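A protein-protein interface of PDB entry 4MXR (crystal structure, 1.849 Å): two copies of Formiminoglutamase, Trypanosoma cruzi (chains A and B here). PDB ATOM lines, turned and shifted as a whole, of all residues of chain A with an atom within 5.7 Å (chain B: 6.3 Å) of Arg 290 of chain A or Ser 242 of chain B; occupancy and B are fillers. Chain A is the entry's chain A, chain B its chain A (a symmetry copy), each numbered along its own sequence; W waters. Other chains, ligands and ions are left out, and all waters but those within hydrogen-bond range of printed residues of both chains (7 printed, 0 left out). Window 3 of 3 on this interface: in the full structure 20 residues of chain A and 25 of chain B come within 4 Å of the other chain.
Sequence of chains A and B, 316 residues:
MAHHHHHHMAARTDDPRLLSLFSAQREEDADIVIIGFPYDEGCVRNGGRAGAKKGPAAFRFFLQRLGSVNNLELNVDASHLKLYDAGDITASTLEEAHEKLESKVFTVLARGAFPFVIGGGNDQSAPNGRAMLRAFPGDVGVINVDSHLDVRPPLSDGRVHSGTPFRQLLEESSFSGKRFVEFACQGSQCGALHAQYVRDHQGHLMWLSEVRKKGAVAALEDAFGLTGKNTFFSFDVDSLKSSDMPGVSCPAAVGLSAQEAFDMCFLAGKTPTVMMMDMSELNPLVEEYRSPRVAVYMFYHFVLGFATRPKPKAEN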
ATOM      1  N   SER A 242     -11.132   5.501  21.079  1.00  0.00           N
ATOM      2  CA  SER A 242     -11.134   6.325  19.875  1.00  0.00           C
ATOM      3  C   SER A 242      -9.725   6.626  19.354  1.00  0.00           C
ATOM      4  O   SER A 242      -9.564   7.136  18.242  1.00  0.00           O
ATOM      5  CB  SER A 242     -11.921   7.627  20.098  1.00  0.00           C
ATOM      6  OG  SER A 242     -11.297   8.439  21.082  1.00  0.00           O
ATOM      7  N   SER A 243      -8.706   6.307  20.148  1.00  0.00           N
ATOM      8  CA  SER A 243      -7.328   6.416  19.672  1.00  0.00           C
ATOM      9  C   SER A 243      -7.090   5.463  18.504  1.00  0.00           C
ATOM     10  O   SER A 243      -6.352   5.790  17.576  1.00  0.00           O
ATOM     11  CB  SER A 243      -6.323   6.153  20.799  1.00  0.00           C
ATOM     12  OG  SER A 243      -6.546   4.886  21.396  1.00  0.00           O
ATOM     13  N   ASP A 244      -7.722   4.288  18.560  1.00  0.00           N
ATOM     14  CA  ASP A 244      -7.682   3.307  17.473  1.00  0.00           C
ATOM     15  C   ASP A 244      -8.885   3.453  16.544  1.00  0.00           C
ATOM     16  O   ASP A 244      -8.775   3.245  15.342  1.00  0.00           O
ATOM     17  CB  ASP A 244      -7.676   1.872  18.020  1.00  0.00           C
ATOM     18  CG  ASP A 244      -6.358   1.491  18.664  1.00  0.00           C
ATOM     19  OD1 ASP A 244      -5.317   2.067  18.286  1.00  0.00           O
ATOM     20  OD2 ASP A 244      -6.363   0.601  19.543  1.00  0.00           O
ATOM     21  N   MET A 245     -10.032   3.805  17.114  1.00  0.00           N
ATOM     22  CA  MET A 245     -11.292   3.796  16.378  1.00  0.00           C
ATOM     23  C   MET A 245     -12.030   5.120  16.547  1.00  0.00           C
ATOM     24  O   MET A 245     -13.025   5.195  17.271  1.00  0.00           O
ATOM     25  CB  MET A 245     -12.168   2.637  16.871  1.00  0.00           C
ATOM     26  CG  MET A 245     -13.371   2.309  15.988  1.00  0.00           C
ATOM     27  SD  MET A 245     -12.851   1.825  14.332  1.00  0.00           S
ATOM     28  CE  MET A 245     -13.843   0.368  14.030  1.00  0.00           C
ATOM     29  N   PRO A 246     -11.542   6.178  15.887  1.00  0.00           N
ATOM     30  CA  PRO A 246     -12.172   7.488  16.091  1.00  0.00           C
ATOM     31  C   PRO A 246     -13.459   7.676  15.288  1.00  0.00           C
ATOM     32  O   PRO A 246     -14.275   8.524  15.649  1.00  0.00           O
ATOM     33  CB  PRO A 246     -11.096   8.475  15.620  1.00  0.00           C
ATOM     34  CG  PRO A 246     -10.254   7.698  14.658  1.00  0.00           C
ATOM     35  CD  PRO A 246     -10.273   6.270  15.141  1.00  0.00           C
ATOM     36  N   GLU A 287     -14.452   9.953  10.790  1.00  0.00           N
ATOM     37  CA  GLU A 287     -13.092   9.628  10.340  1.00  0.00           C
ATOM     38  C   GLU A 287     -13.173   8.509   9.299  1.00  0.00           C
ATOM     39  O   GLU A 287     -13.812   7.486   9.541  1.00  0.00           O
ATOM     40  CB  GLU A 287     -12.193   9.231  11.518  1.00  0.00           C
ATOM     41  CG  GLU A 287     -10.693   9.207  11.200  1.00  0.00           C
ATOM     42  CD  GLU A 287     -10.257   7.946  10.468  1.00  0.00           C
ATOM     43  OE1 GLU A 287     -10.812   6.868  10.765  1.00  0.00           O
ATOM     44  OE2 GLU A 287      -9.353   8.029   9.607  1.00  0.00           O
ATOM     45  N   GLU A 288     -12.530   8.701   8.147  1.00  0.00           N
ATOM     46  CA  GLU A 288     -12.846   7.889   6.967  1.00  0.00           C
ATOM     47  C   GLU A 288     -11.781   6.903   6.481  1.00  0.00           C
ATOM     48  O   GLU A 288     -12.035   6.127   5.557  1.00  0.00           O
ATOM     49  CB  GLU A 288     -13.252   8.794   5.798  1.00  0.00           C
ATOM     50  CG  GLU A 288     -12.099   9.562   5.189  1.00  0.00           C
ATOM     51  CD  GLU A 288     -12.485  10.274   3.907  1.00  0.00           C
ATOM     52  OE1 GLU A 288     -11.695  11.120   3.437  1.00  0.00           O
ATOM     53  OE2 GLU A 288     -13.577   9.988   3.369  1.00  0.00           O
ATOM     54  N   TYR A 289     -10.599   6.921   7.081  1.00  0.00           N
ATOM     55  CA  TYR A 289      -9.526   6.064   6.585  1.00  0.00           C
ATOM     56  C   TYR A 289      -9.125   4.986   7.586  1.00  0.00           C
ATOM     57  O   TYR A 289      -9.202   3.788   7.298  1.00  0.00           O
ATOM     58  CB  TYR A 289      -8.303   6.896   6.196  1.00  0.00           C
ATOM     59  CG  TYR A 289      -7.382   6.200   5.212  1.00  0.00           C
ATOM     60  CD1 TYR A 289      -7.574   6.330   3.843  1.00  0.00           C
ATOM     61  CD2 TYR A 289      -6.324   5.412   5.654  1.00  0.00           C
ATOM     62  CE1 TYR A 289      -6.738   5.697   2.938  1.00  0.00           C
ATOM     63  CE2 TYR A 289      -5.483   4.772   4.758  1.00  0.00           C
ATOM     64  CZ  TYR A 289      -5.694   4.918   3.401  1.00  0.00           C
ATOM     65  OH  TYR A 289      -4.862   4.289   2.500  1.00  0.00           O
ATOM     66  N   ARG A 290      -8.698   5.420   8.764  1.00  0.00           N
ATOM     67  CA  ARG A 290      -8.183   4.499   9.769  1.00  0.00           C
ATOM     68  C   ARG A 290      -9.281   3.591  10.324  1.00  0.00           C
ATOM     69  O   ARG A 290      -9.067   2.397  10.543  1.00  0.00           O
ATOM     70  CB  ARG A 290      -7.511   5.289  10.899  1.00  0.00           C
ATOM     71  CG  ARG A 290      -6.301   6.101  10.442  1.00  0.00           C
ATOM     72  CD  ARG A 290      -5.720   6.938  11.585  1.00  0.00           C
ATOM     73  NE  ARG A 290      -5.360   6.089  12.715  1.00  0.00           N
ATOM     74  CZ  ARG A 290      -5.793   6.263  13.957  1.00  0.00           C
ATOM     75  NH1 ARG A 290      -6.598   7.275  14.248  1.00  0.00           N
ATOM     76  NH2 ARG A 290      -5.410   5.423  14.909  1.00  0.00           N
ATOM     77  N   SER A 291     -10.458   4.161  10.548  1.00  0.00           N
ATOM     78  CA  SER A 291     -11.531   3.436  11.218  1.00  0.00           C
ATOM     79  C   SER A 291     -12.137   2.318  10.368  1.00  0.00           C
ATOM     80  O   SER A 291     -12.285   1.193  10.848  1.00  0.00           O
ATOM     81  CB  SER A 291     -12.592   4.404  11.742  1.00  0.00           C
ATOM     82  OG  SER A 291     -11.987   5.341  12.619  1.00  0.00           O
ATOM     83  N   PRO A 292     -12.479   2.614   9.102  1.00  0.00           N
ATOM     84  CA  PRO A 292     -12.939   1.525   8.230  1.00  0.00           C
ATOM     85  C   PRO A 292     -11.905   0.404   8.075  1.00  0.00           C
ATOM     86  O   PRO A 292     -12.272  -0.766   7.970  1.00  0.00           O
ATOM     87  CB  PRO A 292     -13.165   2.233   6.892  1.00  0.00           C
ATOM     88  CG  PRO A 292     -13.496   3.645   7.279  1.00  0.00           C
ATOM     89  CD  PRO A 292     -12.615   3.932   8.456  1.00  0.00           C
ATOM     90  N   ARG A 293     -10.623   0.755   8.062  1.00  0.00           N
ATOM     91  CA  ARG A 293      -9.574  -0.259   7.979  1.00  0.00           C
ATOM     92  C   ARG A 293      -9.621  -1.178   9.196  1.00  0.00           C
ATOM     93  O   ARG A 293      -9.525  -2.400   9.075  1.00  0.00           O
ATOM     94  CB  ARG A 293      -8.196   0.391   7.818  1.00  0.00           C
ATOM     95  CG  ARG A 293      -7.979   0.997   6.433  1.00  0.00           C
ATOM     96  CD  ARG A 293      -6.757   1.911   6.375  1.00  0.00           C
ATOM     97  NE  ARG A 293      -5.499   1.179   6.467  1.00  0.00           N
ATOM     98  CZ  ARG A 293      -4.832   0.700   5.420  1.00  0.00           C
ATOM     99  NH1 ARG A 293      -5.302   0.878   4.193  1.00  0.00           N
ATOM    100  NH2 ARG A 293      -3.690   0.049   5.599  1.00  0.00           N
ATOM    101  N   VAL A 294      -9.783  -0.593  10.375  1.00  0.00           N
ATOM    102  CA  VAL A 294      -9.926  -1.400  11.585  1.00  0.00           C
ATOM    103  C   VAL A 294     -11.140  -2.318  11.487  1.00  0.00           C
ATOM    104  O   VAL A 294     -11.071  -3.505  11.827  1.00  0.00           O
ATOM    105  CB  VAL A 294     -10.039  -0.518  12.835  1.00  0.00           C
ATOM    106  CG1 VAL A 294     -10.486  -1.350  14.037  1.00  0.00           C
ATOM    107  CG2 VAL A 294      -8.700   0.164  13.103  1.00  0.00           C
ATOM    108  N   ALA A 295     -12.252  -1.762  11.015  1.00  0.00           N
ATOM    109  CA  ALA A 295     -13.485  -2.528  10.854  1.00  0.00           C
ATOM    110  C   ALA A 295     -13.280  -3.717   9.917  1.00  0.00           C
ATOM    111  O   ALA A 295     -13.748  -4.819  10.189  1.00  0.00           O
ATOM    112  CB  ALA A 295     -14.602  -1.638  10.340  1.00  0.00           C
ATOM    113  N   LEU B 240       4.769   1.272  13.359  1.00  0.00           N
ATOM    114  CA  LEU B 240       4.120   1.800  14.552  1.00  0.00           C
ATOM    115  C   LEU B 240       2.609   1.896  14.355  1.00  0.00           C
ATOM    116  O   LEU B 240       2.134   2.254  13.272  1.00  0.00           O
ATOM    117  CB  LEU B 240       4.677   3.187  14.917  1.00  0.00           C
ATOM    118  CG  LEU B 240       6.027   3.271  15.631  1.00  0.00           C
ATOM    119  CD1 LEU B 240       7.158   2.808  14.723  1.00  0.00           C
ATOM    120  CD2 LEU B 240       6.274   4.696  16.119  1.00  0.00           C
ATOM    121  N   LYS B 241       1.857   1.581  15.407  1.00  0.00           N
ATOM    122  CA  LYS B 241       0.408   1.746  15.377  1.00  0.00           C
ATOM    123  C   LYS B 241       0.065   3.185  14.997  1.00  0.00           C
ATOM    124  O   LYS B 241       0.691   4.130  15.480  1.00  0.00           O
ATOM    125  CB  LYS B 241      -0.198   1.390  16.743  1.00  0.00           C
ATOM    126  CG  LYS B 241       0.311   2.251  17.899  1.00  0.00           C
ATOM    127  CD  LYS B 241       0.231   1.497  19.224  1.00  0.00           C
ATOM    128  CE  LYS B 241      -1.193   1.101  19.564  1.00  0.00           C
ATOM    129  NZ  LYS B 241      -1.243   0.145  20.716  1.00  0.00           N
ATOM    130  N   SER B 242      -0.921   3.351  14.123  1.00  0.00           N
ATOM    131  CA  SER B 242      -1.259   4.674  13.607  1.00  0.00           C
ATOM    132  C   SER B 242      -1.876   5.590  14.670  1.00  0.00           C
ATOM    133  O   SER B 242      -2.028   6.794  14.446  1.00  0.00           O
ATOM    134  CB  SER B 242      -2.177   4.570  12.378  1.00  0.00           C
ATOM    135  OG  SER B 242      -3.428   3.995  12.722  1.00  0.00           O
ATOM    136  N   SER B 243      -2.225   5.027  15.824  1.00  0.00           N
ATOM    137  CA  SER B 243      -2.678   5.848  16.946  1.00  0.00           C
ATOM    138  C   SER B 243      -1.563   6.781  17.407  1.00  0.00           C
ATOM    139  O   SER B 243      -1.826   7.915  17.804  1.00  0.00           O
ATOM    140  CB  SER B 243      -3.176   4.982  18.108  1.00  0.00           C
ATOM    141  OG  SER B 243      -2.176   4.069  18.530  1.00  0.00           O
ATOM    142  N   ASP B 244      -0.320   6.293  17.351  1.00  0.00           N
ATOM    143  CA  ASP B 244       0.867   7.094  17.659  1.00  0.00           C
ATOM    144  C   ASP B 244       1.478   7.696  16.396  1.00  0.00           C
ATOM    145  O   ASP B 244       2.001   8.804  16.421  1.00  0.00           O
ATOM    146  CB  ASP B 244       1.946   6.245  18.350  1.00  0.00           C
ATOM    147  CG  ASP B 244       1.588   5.885  19.778  1.00  0.00           C
ATOM    148  OD1 ASP B 244       0.821   6.639  20.413  1.00  0.00           O
ATOM    149  OD2 ASP B 244       2.088   4.850  20.271  1.00  0.00           O
ATOM    150  N   MET B 245       1.413   6.954  15.296  1.00  0.00           N
ATOM    151  CA  MET B 245       2.119   7.324  14.074  1.00  0.00           C
ATOM    152  C   MET B 245       1.181   7.289  12.872  1.00  0.00           C
ATOM    153  O   MET B 245       1.252   6.376  12.048  1.00  0.00           O
ATOM    154  CB  MET B 245       3.297   6.368  13.851  1.00  0.00           C
ATOM    155  CG  MET B 245       4.309   6.816  12.797  1.00  0.00           C
ATOM    156  SD  MET B 245       5.065   8.389  13.245  1.00  0.00           S
ATOM    157  CE  MET B 245       6.800   8.080  12.939  1.00  0.00           C
ATOM    158  N   PRO B 246       0.286   8.279  12.768  1.00  0.00           N
ATOM    159  CA  PRO B 246      -0.692   8.236  11.675  1.00  0.00           C
ATOM    160  C   PRO B 246      -0.127   8.708  10.335  1.00  0.00           C
ATOM    161  O   PRO B 246      -0.680   8.362   9.292  1.00  0.00           O
ATOM    162  CB  PRO B 246      -1.801   9.182  12.152  1.00  0.00           C
ATOM    163  CG  PRO B 246      -1.127  10.115  13.107  1.00  0.00           C
ATOM    164  CD  PRO B 246      -0.026   9.322  13.765  1.00  0.00           C
ATOM    165  N   GLY B 247       0.960   9.474  10.369  1.00  0.00           N
ATOM    166  CA  GLY B 247       1.469  10.139   9.181  1.00  0.00           C
ATOM    167  C   GLY B 247       2.354   9.265   8.319  1.00  0.00           C
ATOM    168  O   GLY B 247       3.543   9.539   8.168  1.00  0.00           O
ATOM    169  N   VAL B 248       1.772   8.209   7.759  1.00  0.00           N
ATOM    170  CA  VAL B 248       2.467   7.323   6.829  1.00  0.00           C
ATOM    171  C   VAL B 248       1.509   6.934   5.710  1.00  0.00           C
ATOM    172  O   VAL B 248       0.292   7.037   5.870  1.00  0.00           O
ATOM    173  CB  VAL B 248       2.940   6.030   7.520  1.00  0.00           C
ATOM    174  CG1 VAL B 248       4.018   6.332   8.546  1.00  0.00           C
ATOM    175  CG2 VAL B 248       1.761   5.311   8.162  1.00  0.00           C
ATOM    176  N   PRO B 251      -1.056   3.362   7.012  1.00  0.00           N
ATOM    177  CA  PRO B 251      -1.267   3.427   8.463  1.00  0.00           C
ATOM    178  C   PRO B 251      -1.551   2.059   9.069  1.00  0.00           C
ATOM    179  O   PRO B 251      -2.413   1.328   8.579  1.00  0.00           O
ATOM    180  CB  PRO B 251      -2.504   4.327   8.607  1.00  0.00           C
ATOM    181  CG  PRO B 251      -2.635   5.036   7.298  1.00  0.00           C
ATOM    182  CD  PRO B 251      -2.097   4.091   6.271  1.00  0.00           C
ATOM    183  N   ALA B 252      -0.837   1.726  10.137  1.00  0.00           N
ATOM    184  CA  ALA B 252      -1.023   0.444  10.800  1.00  0.00           C
ATOM    185  C   ALA B 252      -2.155   0.538  11.817  1.00  0.00           C
ATOM    186  O   ALA B 252      -2.205   1.475  12.611  1.00  0.00           O
ATOM    187  CB  ALA B 252       0.272   0.011  11.475  1.00  0.00           C
ATOM    188  N   ALA B 253      -3.074  -0.421  11.789  1.00  0.00           N
ATOM    189  CA  ALA B 253      -4.124  -0.469  12.805  1.00  0.00           C
ATOM    190  C   ALA B 253      -3.492  -0.847  14.141  1.00  0.00           C
ATOM    191  O   ALA B 253      -3.745  -0.218  15.168  1.00  0.00           O
ATOM    192  CB  ALA B 253      -5.205  -1.475  12.416  1.00  0.00           C
ATOM    193  N   VAL B 254      -2.673  -1.892  14.107  1.00  0.00           N
ATOM    194  CA  VAL B 254      -1.897  -2.331  15.256  1.00  0.00           C
ATOM    195  C   VAL B 254      -0.414  -2.217  14.907  1.00  0.00           C
ATOM    196  O   VAL B 254      -0.059  -2.029  13.741  1.00  0.00           O
ATOM    197  CB  VAL B 254      -2.245  -3.785  15.637  1.00  0.00           C
ATOM    198  CG1 VAL B 254      -3.688  -3.875  16.121  1.00  0.00           C
ATOM    199  CG2 VAL B 254      -2.024  -4.717  14.453  1.00  0.00           C
ATOM    200  N   GLY B 255       0.452  -2.324  15.908  1.00  0.00           N
ATOM    201  CA  GLY B 255       1.878  -2.200  15.678  1.00  0.00           C
ATOM    202  C   GLY B 255       2.622  -1.707  16.903  1.00  0.00           C
ATOM    203  O   GLY B 255       2.083  -1.704  18.014  1.00  0.00           O
ATOM    204  N   LEU B 256       3.868  -1.288  16.703  1.00  0.00           N
ATOM    205  CA  LEU B 256       4.705  -0.826  17.807  1.00  0.00           C
ATOM    206  C   LEU B 256       4.202   0.495  18.374  1.00  0.00           C
ATOM    207  O   LEU B 256       3.700   1.342  17.640  1.00  0.00           O
ATOM    208  CB  LEU B 256       6.159  -0.676  17.345  1.00  0.00           C
ATOM    209  CG  LEU B 256       6.822  -1.953  16.821  1.00  0.00           C
ATOM    210  CD1 LEU B 256       8.083  -1.636  16.027  1.00  0.00           C
ATOM    211  CD2 LEU B 256       7.118  -2.914  17.970  1.00  0.00           C
ATOM    212  N   ARG B 290       2.160  15.508  14.678  1.00  0.00           N
ATOM    213  CA  ARG B 290       2.456  14.479  15.666  1.00  0.00           C
ATOM    214  C   ARG B 290       3.478  13.467  15.146  1.00  0.00           C
ATOM    215  O   ARG B 290       4.372  13.035  15.876  1.00  0.00           O
ATOM    216  CB  ARG B 290       1.159  13.773  16.082  1.00  0.00           C
ATOM    217  CG  ARG B 290       0.149  14.697  16.757  1.00  0.00           C
ATOM    218  CD  ARG B 290      -1.160  13.968  17.073  1.00  0.00           C
ATOM    219  NE  ARG B 290      -0.909  12.799  17.910  1.00  0.00           N
ATOM    220  CZ  ARG B 290      -1.296  11.564  17.615  1.00  0.00           C
ATOM    221  NH1 ARG B 290      -1.975  11.325  16.503  1.00  0.00           N
ATOM    222  NH2 ARG B 290      -1.005  10.571  18.444  1.00  0.00           N
HETATM  223  O   HOH W   1      -6.423   2.631  13.745  1.00  0.00           O
HETATM  224  O   HOH W   2      -2.363  -1.710   7.562  1.00  0.00           O
HETATM  225  O   HOH W   3      -4.089   0.370  21.141  1.00  0.00           O
HETATM  226  O   HOH W   4      -4.949   0.579   9.239  1.00  0.00           O
HETATM  227  O   HOH W   5      -4.395   3.420  20.772  1.00  0.00           O
HETATM  228  O   HOH W   6      -4.144   2.484  15.724  1.00  0.00           O
HETATM  229  O   HOH W   7      -3.561  -0.273  17.983  1.00  0.00           O
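Ser 243 of chain A touches its own counterpart, Ser 243 of chain B. Asp 244 of chain A touches Ser 243 of chain B, but with the chains exchanged Ser 243 of chain A does not touch Asp 244 of chain B (6.1 Å). Arg 290 of chain A touches Ser 242 of chain B, but with the chains exchanged Ser 242 of chain A does not touch Arg 290 of chain B (8.8 Å). Arg 290 of chain A touches Ser 243 of chain B, but with the chains exchanged Ser 243 of chain A does not touch Arg 290 of chain B (7.1 Å). Positions printed for both chains: 242, 243, 244, 245, 246 and 290. Of the 7 pairs that touch across the chains among the printed residues, 1 has its exchanged pair printed and touching as well.
Of chain B, only Ser 242 and Ser 243 come within 4 Å of Arg 290 of chain A. Of chain A, only Arg 290 (2.8 Å) comes within 4 Å of Ser 242 of chain B. Printed residues of chain B within 4 Å of Val 294 of chain A: Ala 253. Of the printed residues of chain B, Tyr 289 of chain A touches Pro 251. Of the printed residues of chain B, Arg 293 of chain A touches Pro 251. Of the printed residues of chain B, Ser 243 of chain A touches Ser 243 (3.3 Å). The nearest printed residue of chain B that does not touch Arg 290 of chain A is Pro 246 of chain B (4.6 Å). The nearest residue of chain A that does not touch Ser 242 of chain B is Ser 243 of chain A (5.3 Å). The nearest printed residue of chain B that does not touch Tyr 289 of chain A is Val 248 of chain B (6.3 Å).
Water W5 lies within hydrogen-bond range of OG of Ser 243 of chain A (2.7 Å), OD1 of Asp 244 of chain A (3.0 Å) and OG of Ser 243 of chain B (3.2 Å). Water W4 lies within hydrogen-bond range of the backbone carbonyl oxygen of Pro 251 of chain B, the guanidinium group of Arg 293 of chain A and the backbone NH of Ala 253 of chain B. Water W6 lies within hydrogen-bond range of the backbone carbonyl oxygen of Ala 253 of chain B (2.8 Å), the side-chain carboxylate of Asp 244 of chain A (2.8 Å), the backbone NH of Ser 243 of chain B (3.2 Å), the guanidinium group of Arg 290 of chain A (3.3 Å) and the side-chain hydroxyl of Ser 242 of chain B (3.4 Å). Water W3 lies within hydrogen-bond range of OD2 of Asp 244 of chain A and NZ of Lys 241 of chain B. Water W7 lies within hydrogen-bond range of the backbone carbonyl oxygen of Ala 253 of chain B (2.8 Å) and the side-chain carboxylate of Asp 244 of chain A (2.9 Å). Water W2 lies within hydrogen-bond range of NH2 of Arg 293 of chain A (3.0 Å) and O of Pro 251 of chain B (3.2 Å).
The backbone carbonyl oxygen (O) of Ala 252 of chain B sits at hydrogen-bond distance from the backbone NH (N) of Ser 242 of chain B (2.7 Å). The backbone NH (N) of Tyr 289 of chain A sits at hydrogen-bond distance from the side-chain carboxylate (OE2) of Glu 287 of chain A, 3.0 Å away. OE2 of Glu 287 of chain A sits at hydrogen-bond distance from N of Arg 290 of chain A (2.8 Å). The guanidinium group of Arg 290 of chain A is in hydrogen-bond range of the backbone carbonyl oxygen of Ser 243 of chain A (2.9 Å). NH2 of Arg 290 of chain B sits at hydrogen-bond distance from O of Ser 243 of chain B, at 2.9 Å.
The side-chain hydroxyl of Ser 242 of chain B sits at hydrogen-bond distance from the guanidinium group of Arg 290 of chain A (2.8 Å). The guanidinium group (NH2) of Arg 293 of chain A is in hydrogen-bond range of the backbone carbonyl oxygen (O) of Pro 251 of chain B, 3.5 Å away. The guanidinium group (NH2) of Arg 290 of chain A sits close to the backbone NH (N) of Ser 243 of chain B (3.3 Å).
Ser 243 of chain A touches Ser 243 of chain B. CB of Ser 243 of chain B touches OD1 of Asp 244 of chain A, at 3.6 Å. CD of Pro 251 of chain B touches CE2 of Tyr 289 of chain A, 3.8 Å away. Ala 253 of chain B touches Val 294 of chain A (CB to CG2, 3.9 Å).
Of the 16 printed residues of chain B, 4 touch a printed residue of chain A. Hydrophobic or aromatic side chains of chain B that line the printed part of chain A: Pro 251 and Ala 253. Of the 14 printed residues of chain A, 6 touch a printed residue of chain B. Printed residues of chain A that touch a printed residue of chain B: Ser 243, Asp 244, Tyr 289, Arg 290, Arg 293 and Val 294. Hydrophobic or aromatic side chains of chain A that line the printed part of chain B: Tyr 289 and Val 294. Along chain A the printed residues that touch a printed residue of chain B span positions 243 to 294. Among the printed residues, 7 pairs touch across the chains.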
